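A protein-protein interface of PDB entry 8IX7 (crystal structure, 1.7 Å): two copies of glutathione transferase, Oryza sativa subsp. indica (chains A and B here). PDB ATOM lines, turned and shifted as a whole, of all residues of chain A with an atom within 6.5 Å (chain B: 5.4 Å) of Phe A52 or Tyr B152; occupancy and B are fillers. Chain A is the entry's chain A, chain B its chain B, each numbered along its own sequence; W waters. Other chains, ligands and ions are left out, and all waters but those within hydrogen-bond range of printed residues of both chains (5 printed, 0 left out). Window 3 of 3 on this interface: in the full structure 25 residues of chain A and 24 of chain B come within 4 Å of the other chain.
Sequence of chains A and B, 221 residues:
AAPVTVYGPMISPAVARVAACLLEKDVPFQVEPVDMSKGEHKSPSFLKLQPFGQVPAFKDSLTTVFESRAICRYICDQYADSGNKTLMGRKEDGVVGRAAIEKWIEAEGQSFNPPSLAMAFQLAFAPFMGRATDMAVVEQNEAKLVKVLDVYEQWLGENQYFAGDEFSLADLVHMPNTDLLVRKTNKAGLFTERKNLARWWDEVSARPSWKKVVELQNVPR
OE1 of Gln A50 sits at hydrogen-bond distance from N of Phe A52 (2.8 Å).
The backbone NH (N) of Phe B112 is in hydrogen-bond range of the backbone carbonyl oxygen (O) of Ala B107.
The side-chain hydroxyl (OH) of Tyr B152 lies within hydrogen-bond range of a ring nitrogen (NE2) of His B174.
Among the printed residues, pairs that only touch across the chains: Pro A51 with Val B151, Phe A52 with Ala B107, Phe A52 with Val B151, Phe A52 with Tyr B152 and Phe A66 with Trp B104.
Printed residues of chain B within 4 Å of Pro A51: Val B151 (3.8 Å).
Printed residues of chain A within 4 Å of Ala B107: Phe A52 (3.9 Å).
Of the printed residues of chain A, Val B151 touches Pro A51 and Phe A52.
Of chain A, only Phe A52 (3.9 Å) comes within 4 Å of Tyr B152.
Trp B155 touches none of the printed residues of chain A.
Asn B196 touches none of the printed residues of chain A.
The nearest printed residue of chain A that does not touch Trp B104 is Phe A52 (4.1 Å).
Of the 10 printed residues of chain A, 3 touch a printed residue of chain B.
Hydrophobic or aromatic side chains of chain A within 4 Å of the printed part of chain B: Pro A51, Phe A52 and Phe A66.
Along chain A the printed residues that touch a printed residue of chain B span positions 51 to 66.
Among the printed residues, no Asp or Glu carboxylate lies within 4 Å of a Lys or Arg side-chain nitrogen of the other chain.
No position is printed for both chains.
Of the 5 pairs that touch across the chains among the printed residues, none has its exchanged pair printed and touching as well.
Water W1 lies within hydrogen-bond range of OE2 of Glu A67 and OG of Ser B111.
Water W4 bridges O of Pro A51 (2.8 Å) and NE2 of Gln B154 (3.5 Å).
Water W3 lies within hydrogen-bond range of OG of Ser B111 (2.8 Å) and NE2 of Gln A54 (3.3 Å).
Water W5 bridges the backbone carbonyl oxygen of Leu A47 (3.0 Å) and the side-chain amide nitrogen of Gln B154 (3.3 Å).
Water W2 lies within hydrogen-bond range of OG of Ser B111 (3.1 Å), OE1 of Gln A54 (3.1 Å) and OE2 of Glu A67 (3.4 Å).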
ATOM      1  N   HIS A  41      -3.655  -2.357  17.977  1.00  0.00           N
ATOM      2  CA  HIS A  41      -4.548  -3.246  17.246  1.00  0.00           C
ATOM      3  C   HIS A  41      -5.352  -4.100  18.219  1.00  0.00           C
ATOM      4  O   HIS A  41      -6.240  -4.855  17.810  1.00  0.00           O
ATOM      5  CB  HIS A  41      -3.746  -4.156  16.313  1.00  0.00           C
ATOM      6  CG  HIS A  41      -2.811  -5.082  17.029  1.00  0.00           C
ATOM      7  ND1 HIS A  41      -1.763  -4.631  17.802  1.00  0.00           N
ATOM      8  CD2 HIS A  41      -2.768  -6.434  17.087  1.00  0.00           C
ATOM      9  CE1 HIS A  41      -1.112  -5.665  18.305  1.00  0.00           C
ATOM     10  NE2 HIS A  41      -1.702  -6.771  17.887  1.00  0.00           N
ATOM     11  N   PHE A  46     -10.197  -0.405  18.450  1.00  0.00           N
ATOM     12  CA  PHE A  46      -9.829  -1.013  17.178  1.00  0.00           C
ATOM     13  C   PHE A  46     -10.559  -2.340  17.025  1.00  0.00           C
ATOM     14  O   PHE A  46     -10.969  -2.710  15.926  1.00  0.00           O
ATOM     15  CB  PHE A  46      -8.324  -1.258  17.088  1.00  0.00           C
ATOM     16  CG  PHE A  46      -7.884  -1.764  15.742  1.00  0.00           C
ATOM     17  CD1 PHE A  46      -7.783  -0.896  14.659  1.00  0.00           C
ATOM     18  CD2 PHE A  46      -7.621  -3.117  15.545  1.00  0.00           C
ATOM     19  CE1 PHE A  46      -7.427  -1.369  13.397  1.00  0.00           C
ATOM     20  CE2 PHE A  46      -7.264  -3.602  14.288  1.00  0.00           C
ATOM     21  CZ  PHE A  46      -7.167  -2.727  13.213  1.00  0.00           C
ATOM     22  N   LEU A  47     -10.718  -3.052  18.136  1.00  0.00           N
ATOM     23  CA  LEU A  47     -11.400  -4.339  18.119  1.00  0.00           C
ATOM     24  C   LEU A  47     -12.871  -4.192  17.740  1.00  0.00           C
ATOM     25  O   LEU A  47     -13.496  -5.140  17.266  1.00  0.00           O
ATOM     26  CB  LEU A  47     -11.259  -5.028  19.481  1.00  0.00           C
ATOM     27  CG  LEU A  47      -9.836  -5.505  19.797  1.00  0.00           C
ATOM     28  CD1 LEU A  47      -9.792  -6.130  21.181  1.00  0.00           C
ATOM     29  CD2 LEU A  47      -9.390  -6.516  18.750  1.00  0.00           C
ATOM     30  N   GLN A  50     -12.358  -4.125  14.017  1.00  0.00           N
ATOM     31  CA  GLN A  50     -11.759  -5.356  13.512  1.00  0.00           C
ATOM     32  C   GLN A  50     -11.678  -6.358  14.661  1.00  0.00           C
ATOM     33  O   GLN A  50     -10.726  -6.349  15.436  1.00  0.00           O
ATOM     34  CB  GLN A  50     -10.357  -5.038  12.983  1.00  0.00           C
ATOM     35  CG  GLN A  50     -10.030  -5.631  11.623  1.00  0.00           C
ATOM     36  CD  GLN A  50      -9.966  -7.144  11.647  1.00  0.00           C
ATOM     37  OE1 GLN A  50      -9.990  -7.759  12.711  1.00  0.00           O
ATOM     38  NE2 GLN A  50      -9.874  -7.752  10.471  1.00  0.00           N
ATOM     39  N   PRO A  51     -12.679  -7.242  14.779  1.00  0.00           N
ATOM     40  CA  PRO A  51     -12.744  -8.255  15.839  1.00  0.00           C
ATOM     41  C   PRO A  51     -11.526  -9.168  15.994  1.00  0.00           C
ATOM     42  O   PRO A  51     -11.310  -9.738  17.066  1.00  0.00           O
ATOM     43  CB  PRO A  51     -14.003  -9.049  15.481  1.00  0.00           C
ATOM     44  CG  PRO A  51     -14.845  -8.055  14.756  1.00  0.00           C
ATOM     45  CD  PRO A  51     -13.838  -7.362  13.876  1.00  0.00           C
ATOM     46  N   PHE A  52     -10.748  -9.317  14.925  1.00  0.00           N
ATOM     47  CA  PHE A  52      -9.570 -10.180  14.947  1.00  0.00           C
ATOM     48  C   PHE A  52      -8.285  -9.441  15.305  1.00  0.00           C
ATOM     49  O   PHE A  52      -7.222 -10.055  15.432  1.00  0.00           O
ATOM     50  CB  PHE A  52      -9.404 -10.861  13.584  1.00  0.00           C
ATOM     51  CG  PHE A  52     -10.438 -11.907  13.305  1.00  0.00           C
ATOM     52  CD1 PHE A  52     -10.266 -13.210  13.761  1.00  0.00           C
ATOM     53  CD2 PHE A  52     -11.602 -11.584  12.614  1.00  0.00           C
ATOM     54  CE1 PHE A  52     -11.243 -14.180  13.535  1.00  0.00           C
ATOM     55  CE2 PHE A  52     -12.584 -12.544  12.384  1.00  0.00           C
ATOM     56  CZ  PHE A  52     -12.404 -13.844  12.845  1.00  0.00           C
ATOM     57  N   GLY A  53      -8.384  -8.124  15.467  1.00  0.00           N
ATOM     58  CA  GLY A  53      -7.207  -7.340  15.795  1.00  0.00           C
ATOM     59  C   GLY A  53      -6.189  -7.377  14.670  1.00  0.00           C
ATOM     60  O   GLY A  53      -4.980  -7.380  14.912  1.00  0.00           O
ATOM     61  N   GLN A  54      -6.676  -7.416  13.435  1.00  0.00           N
ATOM     62  CA  GLN A  54      -5.808  -7.449  12.263  1.00  0.00           C
ATOM     63  C   GLN A  54      -6.116  -6.242  11.379  1.00  0.00           C
ATOM     64  O   GLN A  54      -7.103  -5.543  11.594  1.00  0.00           O
ATOM     65  CB  GLN A  54      -6.033  -8.750  11.477  1.00  0.00           C
ATOM     66  CG  GLN A  54      -5.861 -10.009  12.325  1.00  0.00           C
ATOM     67  CD  GLN A  54      -6.056 -11.299  11.540  1.00  0.00           C
ATOM     68  OE1 GLN A  54      -6.943 -11.402  10.696  1.00  0.00           O
ATOM     69  NE2 GLN A  54      -5.233 -12.299  11.835  1.00  0.00           N
ATOM     70  N   PHE A  66     -14.783  -5.265   7.875  1.00  0.00           N
ATOM     71  CA  PHE A  66     -13.435  -5.812   8.027  1.00  0.00           C
ATOM     72  C   PHE A  66     -13.221  -6.942   7.013  1.00  0.00           C
ATOM     73  O   PHE A  66     -14.188  -7.433   6.423  1.00  0.00           O
ATOM     74  CB  PHE A  66     -13.170  -6.270   9.477  1.00  0.00           C
ATOM     75  CG  PHE A  66     -13.965  -7.465   9.916  1.00  0.00           C
ATOM     76  CD1 PHE A  66     -13.489  -8.756   9.695  1.00  0.00           C
ATOM     77  CD2 PHE A  66     -15.178  -7.301  10.578  1.00  0.00           C
ATOM     78  CE1 PHE A  66     -14.212  -9.866  10.129  1.00  0.00           C
ATOM     79  CE2 PHE A  66     -15.909  -8.404  11.015  1.00  0.00           C
ATOM     80  CZ  PHE A  66     -15.423  -9.690  10.789  1.00  0.00           C
ATOM     81  N   GLU A  67     -11.954  -7.319   6.817  1.00  0.00           N
ATOM     82  CA  GLU A  67     -11.511  -8.337   5.848  1.00  0.00           C
ATOM     83  C   GLU A  67     -11.432  -7.658   4.480  1.00  0.00           C
ATOM     84  O   GLU A  67     -12.448  -7.254   3.914  1.00  0.00           O
ATOM     85  CB  GLU A  67     -12.459  -9.544   5.803  1.00  0.00           C
ATOM     86  CG  GLU A  67     -12.097 -10.672   6.787  1.00  0.00           C
ATOM     87  CD  GLU A  67     -10.701 -11.258   6.557  1.00  0.00           C
ATOM     88  OE1 GLU A  67     -10.191 -11.195   5.419  1.00  0.00           O
ATOM     89  OE2 GLU A  67     -10.112 -11.801   7.521  1.00  0.00           O
ATOM     90  N   TRP B 104     -18.088 -11.837   7.475  1.00  0.00           N
ATOM     91  CA  TRP B 104     -17.985 -13.116   8.160  1.00  0.00           C
ATOM     92  C   TRP B 104     -17.790 -14.270   7.177  1.00  0.00           C
ATOM     93  O   TRP B 104     -17.262 -15.315   7.549  1.00  0.00           O
ATOM     94  CB  TRP B 104     -19.202 -13.348   9.064  1.00  0.00           C
ATOM     95  CG  TRP B 104     -19.252 -12.350  10.199  1.00  0.00           C
ATOM     96  CD1 TRP B 104     -20.096 -11.284  10.314  1.00  0.00           C
ATOM     97  CD2 TRP B 104     -18.361 -12.281  11.321  1.00  0.00           C
ATOM     98  NE1 TRP B 104     -19.784 -10.549  11.435  1.00  0.00           N
ATOM     99  CE2 TRP B 104     -18.724 -11.138  12.072  1.00  0.00           C
ATOM    100  CE3 TRP B 104     -17.290 -13.072  11.765  1.00  0.00           C
ATOM    101  CZ2 TRP B 104     -18.054 -10.763  13.241  1.00  0.00           C
ATOM    102  CZ3 TRP B 104     -16.622 -12.700  12.933  1.00  0.00           C
ATOM    103  CH2 TRP B 104     -17.009 -11.552  13.658  1.00  0.00           C
ATOM    104  N   ALA B 107     -14.266 -14.175   6.965  1.00  0.00           N
ATOM    105  CA  ALA B 107     -13.648 -14.711   8.172  1.00  0.00           C
ATOM    106  C   ALA B 107     -13.620 -16.235   8.048  1.00  0.00           C
ATOM    107  O   ALA B 107     -12.653 -16.888   8.441  1.00  0.00           O
ATOM    108  CB  ALA B 107     -14.444 -14.294   9.406  1.00  0.00           C
ATOM    109  N   GLU B 108     -14.683 -16.804   7.496  1.00  0.00           N
ATOM    110  CA  GLU B 108     -14.739 -18.257   7.322  1.00  0.00           C
ATOM    111  C   GLU B 108     -13.652 -18.744   6.372  1.00  0.00           C
ATOM    112  O   GLU B 108     -12.895 -19.664   6.689  1.00  0.00           O
ATOM    113  CB  GLU B 108     -16.106 -18.676   6.766  1.00  0.00           C
ATOM    114  CG  GLU B 108     -16.273 -20.187   6.518  1.00  0.00           C
ATOM    115  CD  GLU B 108     -15.805 -20.626   5.137  1.00  0.00           C
ATOM    116  OE1 GLU B 108     -16.088 -19.904   4.151  1.00  0.00           O
ATOM    117  OE2 GLU B 108     -15.170 -21.703   5.030  1.00  0.00           O
ATOM    118  N   SER B 111      -9.891 -17.234   8.007  1.00  0.00           N
ATOM    119  CA  SER B 111      -9.444 -17.569   9.359  1.00  0.00           C
ATOM    120  C   SER B 111      -9.906 -18.915   9.897  1.00  0.00           C
ATOM    121  O   SER B 111      -9.118 -19.660  10.481  1.00  0.00           O
ATOM    122  CB  SER B 111      -9.885 -16.478  10.338  1.00  0.00           C
ATOM    123  OG  SER B 111      -9.280 -15.239  10.014  1.00  0.00           O
ATOM    124  N   PHE B 112     -11.186 -19.208   9.706  1.00  0.00           N
ATOM    125  CA  PHE B 112     -11.783 -20.450  10.192  1.00  0.00           C
ATOM    126  C   PHE B 112     -11.456 -21.701   9.368  1.00  0.00           C
ATOM    127  O   PHE B 112     -11.085 -22.738   9.920  1.00  0.00           O
ATOM    128  CB  PHE B 112     -13.301 -20.267  10.248  1.00  0.00           C
ATOM    129  CG  PHE B 112     -14.052 -21.469  10.756  1.00  0.00           C
ATOM    130  CD1 PHE B 112     -14.174 -21.710  12.120  1.00  0.00           C
ATOM    131  CD2 PHE B 112     -14.673 -22.339   9.864  1.00  0.00           C
ATOM    132  CE1 PHE B 112     -14.910 -22.800  12.590  1.00  0.00           C
ATOM    133  CE2 PHE B 112     -15.409 -23.431  10.321  1.00  0.00           C
ATOM    134  CZ  PHE B 112     -15.530 -23.661  11.685  1.00  0.00           C
ATOM    135  N   VAL B 148      -9.763 -18.348  16.754  1.00  0.00           N
ATOM    136  CA  VAL B 148     -10.878 -17.895  15.933  1.00  0.00           C
ATOM    137  C   VAL B 148     -12.188 -18.121  16.678  1.00  0.00           C
ATOM    138  O   VAL B 148     -13.068 -17.262  16.676  1.00  0.00           O
ATOM    139  CB  VAL B 148     -10.935 -18.653  14.585  1.00  0.00           C
ATOM    140  CG1 VAL B 148     -12.129 -18.160  13.753  1.00  0.00           C
ATOM    141  CG2 VAL B 148      -9.634 -18.443  13.814  1.00  0.00           C
ATOM    142  N   LEU B 149     -12.311 -19.274  17.329  1.00  0.00           N
ATOM    143  CA  LEU B 149     -13.534 -19.578  18.055  1.00  0.00           C
ATOM    144  C   LEU B 149     -13.757 -18.619  19.227  1.00  0.00           C
ATOM    145  O   LEU B 149     -14.901 -18.349  19.589  1.00  0.00           O
ATOM    146  CB  LEU B 149     -13.527 -21.036  18.531  1.00  0.00           C
ATOM    147  CG  LEU B 149     -13.482 -22.076  17.401  1.00  0.00           C
ATOM    148  CD1 LEU B 149     -13.563 -23.487  17.983  1.00  0.00           C
ATOM    149  CD2 LEU B 149     -14.634 -21.833  16.435  1.00  0.00           C
ATOM    150  N   ASP B 150     -12.673 -18.101  19.809  1.00  0.00           N
ATOM    151  CA  ASP B 150     -12.797 -17.154  20.917  1.00  0.00           C
ATOM    152  C   ASP B 150     -13.460 -15.883  20.385  1.00  0.00           C
ATOM    153  O   ASP B 150     -14.276 -15.263  21.070  1.00  0.00           O
ATOM    154  CB  ASP B 150     -11.427 -16.784  21.510  1.00  0.00           C
ATOM    155  CG  ASP B 150     -10.804 -17.910  22.321  1.00  0.00           C
ATOM    156  OD1 ASP B 150     -11.548 -18.747  22.868  1.00  0.00           O
ATOM    157  OD2 ASP B 150      -9.558 -17.940  22.427  1.00  0.00           O
ATOM    158  N   VAL B 151     -13.098 -15.497  19.164  1.00  0.00           N
ATOM    159  CA  VAL B 151     -13.678 -14.307  18.541  1.00  0.00           C
ATOM    160  C   VAL B 151     -15.154 -14.550  18.244  1.00  0.00           C
ATOM    161  O   VAL B 151     -15.998 -13.687  18.496  1.00  0.00           O
ATOM    162  CB  VAL B 151     -12.945 -13.952  17.231  1.00  0.00           C
ATOM    163  CG1 VAL B 151     -13.702 -12.858  16.481  1.00  0.00           C
ATOM    164  CG2 VAL B 151     -11.526 -13.498  17.544  1.00  0.00           C
ATOM    165  N   TYR B 152     -15.456 -15.733  17.714  1.00  0.00           N
ATOM    166  CA  TYR B 152     -16.831 -16.108  17.386  1.00  0.00           C
ATOM    167  C   TYR B 152     -17.713 -16.210  18.628  1.00  0.00           C
ATOM    168  O   TYR B 152     -18.871 -15.782  18.617  1.00  0.00           O
ATOM    169  CB  TYR B 152     -16.855 -17.454  16.651  1.00  0.00           C
ATOM    170  CG  TYR B 152     -16.330 -17.424  15.230  1.00  0.00           C
ATOM    171  CD1 TYR B 152     -15.908 -16.229  14.635  1.00  0.00           C
ATOM    172  CD2 TYR B 152     -16.287 -18.589  14.465  1.00  0.00           C
ATOM    173  CE1 TYR B 152     -15.461 -16.199  13.310  1.00  0.00           C
ATOM    174  CE2 TYR B 152     -15.845 -18.570  13.142  1.00  0.00           C
ATOM    175  CZ  TYR B 152     -15.436 -17.371  12.571  1.00  0.00           C
ATOM    176  OH  TYR B 152     -15.031 -17.347  11.257  1.00  0.00           O
ATOM    177  N   GLU B 153     -17.164 -16.788  19.693  1.00  0.00           N
ATOM    178  CA  GLU B 153     -17.904 -16.952  20.938  1.00  0.00           C
ATOM    179  C   GLU B 153     -18.354 -15.588  21.447  1.00  0.00           C
ATOM    180  O   GLU B 153     -19.499 -15.411  21.852  1.00  0.00           O
ATOM    181  CB  GLU B 153     -17.024 -17.652  21.982  1.00  0.00           C
ATOM    182  CG  GLU B 153     -17.682 -17.877  23.347  1.00  0.00           C
ATOM    183  CD  GLU B 153     -18.896 -18.789  23.288  1.00  0.00           C
ATOM    184  OE1 GLU B 153     -19.083 -19.479  22.262  1.00  0.00           O
ATOM    185  OE2 GLU B 153     -19.660 -18.822  24.279  1.00  0.00           O
ATOM    186  N   GLN B 154     -17.448 -14.620  21.408  1.00  0.00           N
ATOM    187  CA  GLN B 154     -17.768 -13.277  21.865  1.00  0.00           C
ATOM    188  C   GLN B 154     -18.845 -12.664  20.981  1.00  0.00           C
ATOM    189  O   GLN B 154     -19.834 -12.117  21.471  1.00  0.00           O
ATOM    190  CB  GLN B 154     -16.515 -12.404  21.828  1.00  0.00           C
ATOM    191  CG  GLN B 154     -16.732 -10.990  22.314  1.00  0.00           C
ATOM    192  CD  GLN B 154     -15.431 -10.232  22.441  1.00  0.00           C
ATOM    193  OE1 GLN B 154     -14.504 -10.679  23.120  1.00  0.00           O
ATOM    194  NE2 GLN B 154     -15.351  -9.073  21.791  1.00  0.00           N
ATOM    195  N   TRP B 155     -18.651 -12.763  19.672  1.00  0.00           N
ATOM    196  CA  TRP B 155     -19.598 -12.207  18.719  1.00  0.00           C
ATOM    197  C   TRP B 155     -20.997 -12.816  18.827  1.00  0.00           C
ATOM    198  O   TRP B 155     -22.002 -12.100  18.807  1.00  0.00           O
ATOM    199  CB  TRP B 155     -19.062 -12.390  17.296  1.00  0.00           C
ATOM    200  CG  TRP B 155     -19.916 -11.741  16.267  1.00  0.00           C
ATOM    201  CD1 TRP B 155     -20.839 -12.344  15.467  1.00  0.00           C
ATOM    202  CD2 TRP B 155     -19.954 -10.345  15.947  1.00  0.00           C
ATOM    203  NE1 TRP B 155     -21.454 -11.409  14.665  1.00  0.00           N
ATOM    204  CE2 TRP B 155     -20.929 -10.174  14.941  1.00  0.00           C
ATOM    205  CE3 TRP B 155     -19.259  -9.221  16.415  1.00  0.00           C
ATOM    206  CZ2 TRP B 155     -21.228  -8.922  14.390  1.00  0.00           C
ATOM    207  CZ3 TRP B 155     -19.555  -7.973  15.866  1.00  0.00           C
ATOM    208  CH2 TRP B 155     -20.533  -7.837  14.864  1.00  0.00           C
ATOM    209  N   LEU B 156     -21.059 -14.137  18.953  1.00  0.00           N
ATOM    210  CA  LEU B 156     -22.331 -14.835  19.038  1.00  0.00           C
ATOM    211  C   LEU B 156     -23.026 -14.688  20.389  1.00  0.00           C
ATOM    212  O   LEU B 156     -24.089 -15.263  20.614  1.00  0.00           O
ATOM    213  CB  LEU B 156     -22.131 -16.314  18.686  1.00  0.00           C
ATOM    214  CG  LEU B 156     -21.734 -16.518  17.217  1.00  0.00           C
ATOM    215  CD1 LEU B 156     -21.316 -17.969  16.965  1.00  0.00           C
ATOM    216  CD2 LEU B 156     -22.908 -16.134  16.325  1.00  0.00           C
ATOM    217  N   GLY B 157     -22.419 -13.916  21.284  1.00  0.00           N
ATOM    218  CA  GLY B 157     -23.017 -13.675  22.585  1.00  0.00           C
ATOM    219  C   GLY B 157     -23.807 -12.382  22.495  1.00  0.00           C
ATOM    220  O   GLY B 157     -24.606 -12.054  23.375  1.00  0.00           O
ATOM    221  N   PHE B 162     -24.440 -14.832  12.711  1.00  0.00           N
ATOM    222  CA  PHE B 162     -23.321 -13.963  12.358  1.00  0.00           C
ATOM    223  C   PHE B 162     -23.721 -12.572  11.885  1.00  0.00           C
ATOM    224  O   PHE B 162     -23.037 -11.597  12.192  1.00  0.00           O
ATOM    225  CB  PHE B 162     -22.444 -14.644  11.310  1.00  0.00           C
ATOM    226  CG  PHE B 162     -21.442 -15.597  11.895  1.00  0.00           C
ATOM    227  CD1 PHE B 162     -20.274 -15.119  12.482  1.00  0.00           C
ATOM    228  CD2 PHE B 162     -21.669 -16.969  11.876  1.00  0.00           C
ATOM    229  CE1 PHE B 162     -19.345 -15.994  13.041  1.00  0.00           C
ATOM    230  CE2 PHE B 162     -20.745 -17.853  12.433  1.00  0.00           C
ATOM    231  CZ  PHE B 162     -19.580 -17.364  13.017  1.00  0.00           C
ATOM    232  N   HIS B 174     -19.923 -21.732   7.290  1.00  0.00           N
ATOM    233  CA  HIS B 174     -19.214 -22.328   8.424  1.00  0.00           C
ATOM    234  C   HIS B 174     -19.702 -23.731   8.769  1.00  0.00           C
ATOM    235  O   HIS B 174     -19.011 -24.493   9.450  1.00  0.00           O
ATOM    236  CB  HIS B 174     -19.389 -21.476   9.688  1.00  0.00           C
ATOM    237  CG  HIS B 174     -18.580 -20.215   9.707  1.00  0.00           C
ATOM    238  ND1 HIS B 174     -19.061 -19.011   9.240  1.00  0.00           N
ATOM    239  CD2 HIS B 174     -17.334 -19.966  10.177  1.00  0.00           C
ATOM    240  CE1 HIS B 174     -18.148 -18.073   9.426  1.00  0.00           C
ATOM    241  NE2 HIS B 174     -17.091 -18.626   9.993  1.00  0.00           N
ATOM    242  N   ASN B 196     -22.163 -19.879  23.636  1.00  0.00           N
ATOM    243  CA  ASN B 196     -22.710 -19.252  22.443  1.00  0.00           C
ATOM    244  C   ASN B 196     -22.566 -20.062  21.160  1.00  0.00           C
ATOM    245  O   ASN B 196     -23.502 -20.124  20.363  1.00  0.00           O
ATOM    246  CB  ASN B 196     -22.112 -17.855  22.279  1.00  0.00           C
ATOM    247  CG  ASN B 196     -22.341 -16.988  23.504  1.00  0.00           C
ATOM    248  OD1 ASN B 196     -23.422 -17.015  24.099  1.00  0.00           O
ATOM    249  ND2 ASN B 196     -21.333 -16.211  23.884  1.00  0.00           N
ATOM    250  N   LEU B 197     -21.405 -20.678  20.957  1.00  0.00           N
ATOM    251  CA  LEU B 197     -21.185 -21.498  19.770  1.00  0.00           C
ATOM    252  C   LEU B 197     -22.092 -22.724  19.818  1.00  0.00           C
ATOM    253  O   LEU B 197     -22.612 -23.158  18.792  1.00  0.00           O
ATOM    254  CB  LEU B 197     -19.721 -21.935  19.680  1.00  0.00           C
ATOM    255  CG  LEU B 197     -18.772 -20.866  19.135  1.00  0.00           C
ATOM    256  CD1 LEU B 197     -17.332 -21.205  19.484  1.00  0.00           C
ATOM    257  CD2 LEU B 197     -18.970 -20.759  17.626  1.00  0.00           C
HETATM  258  O   HOH W   1     -10.936 -13.181   9.478  1.00  0.00           O
HETATM  259  O   HOH W   2      -7.310 -13.515   8.397  1.00  0.00           O
HETATM  260  O   HOH W   3      -7.219 -14.888  11.867  1.00  0.00           O
HETATM  261  O   HOH W   4     -13.084  -9.525  19.198  1.00  0.00           O
HETATM  262  O   HOH W   5     -14.655  -7.083  19.189  1.00  0.00           O
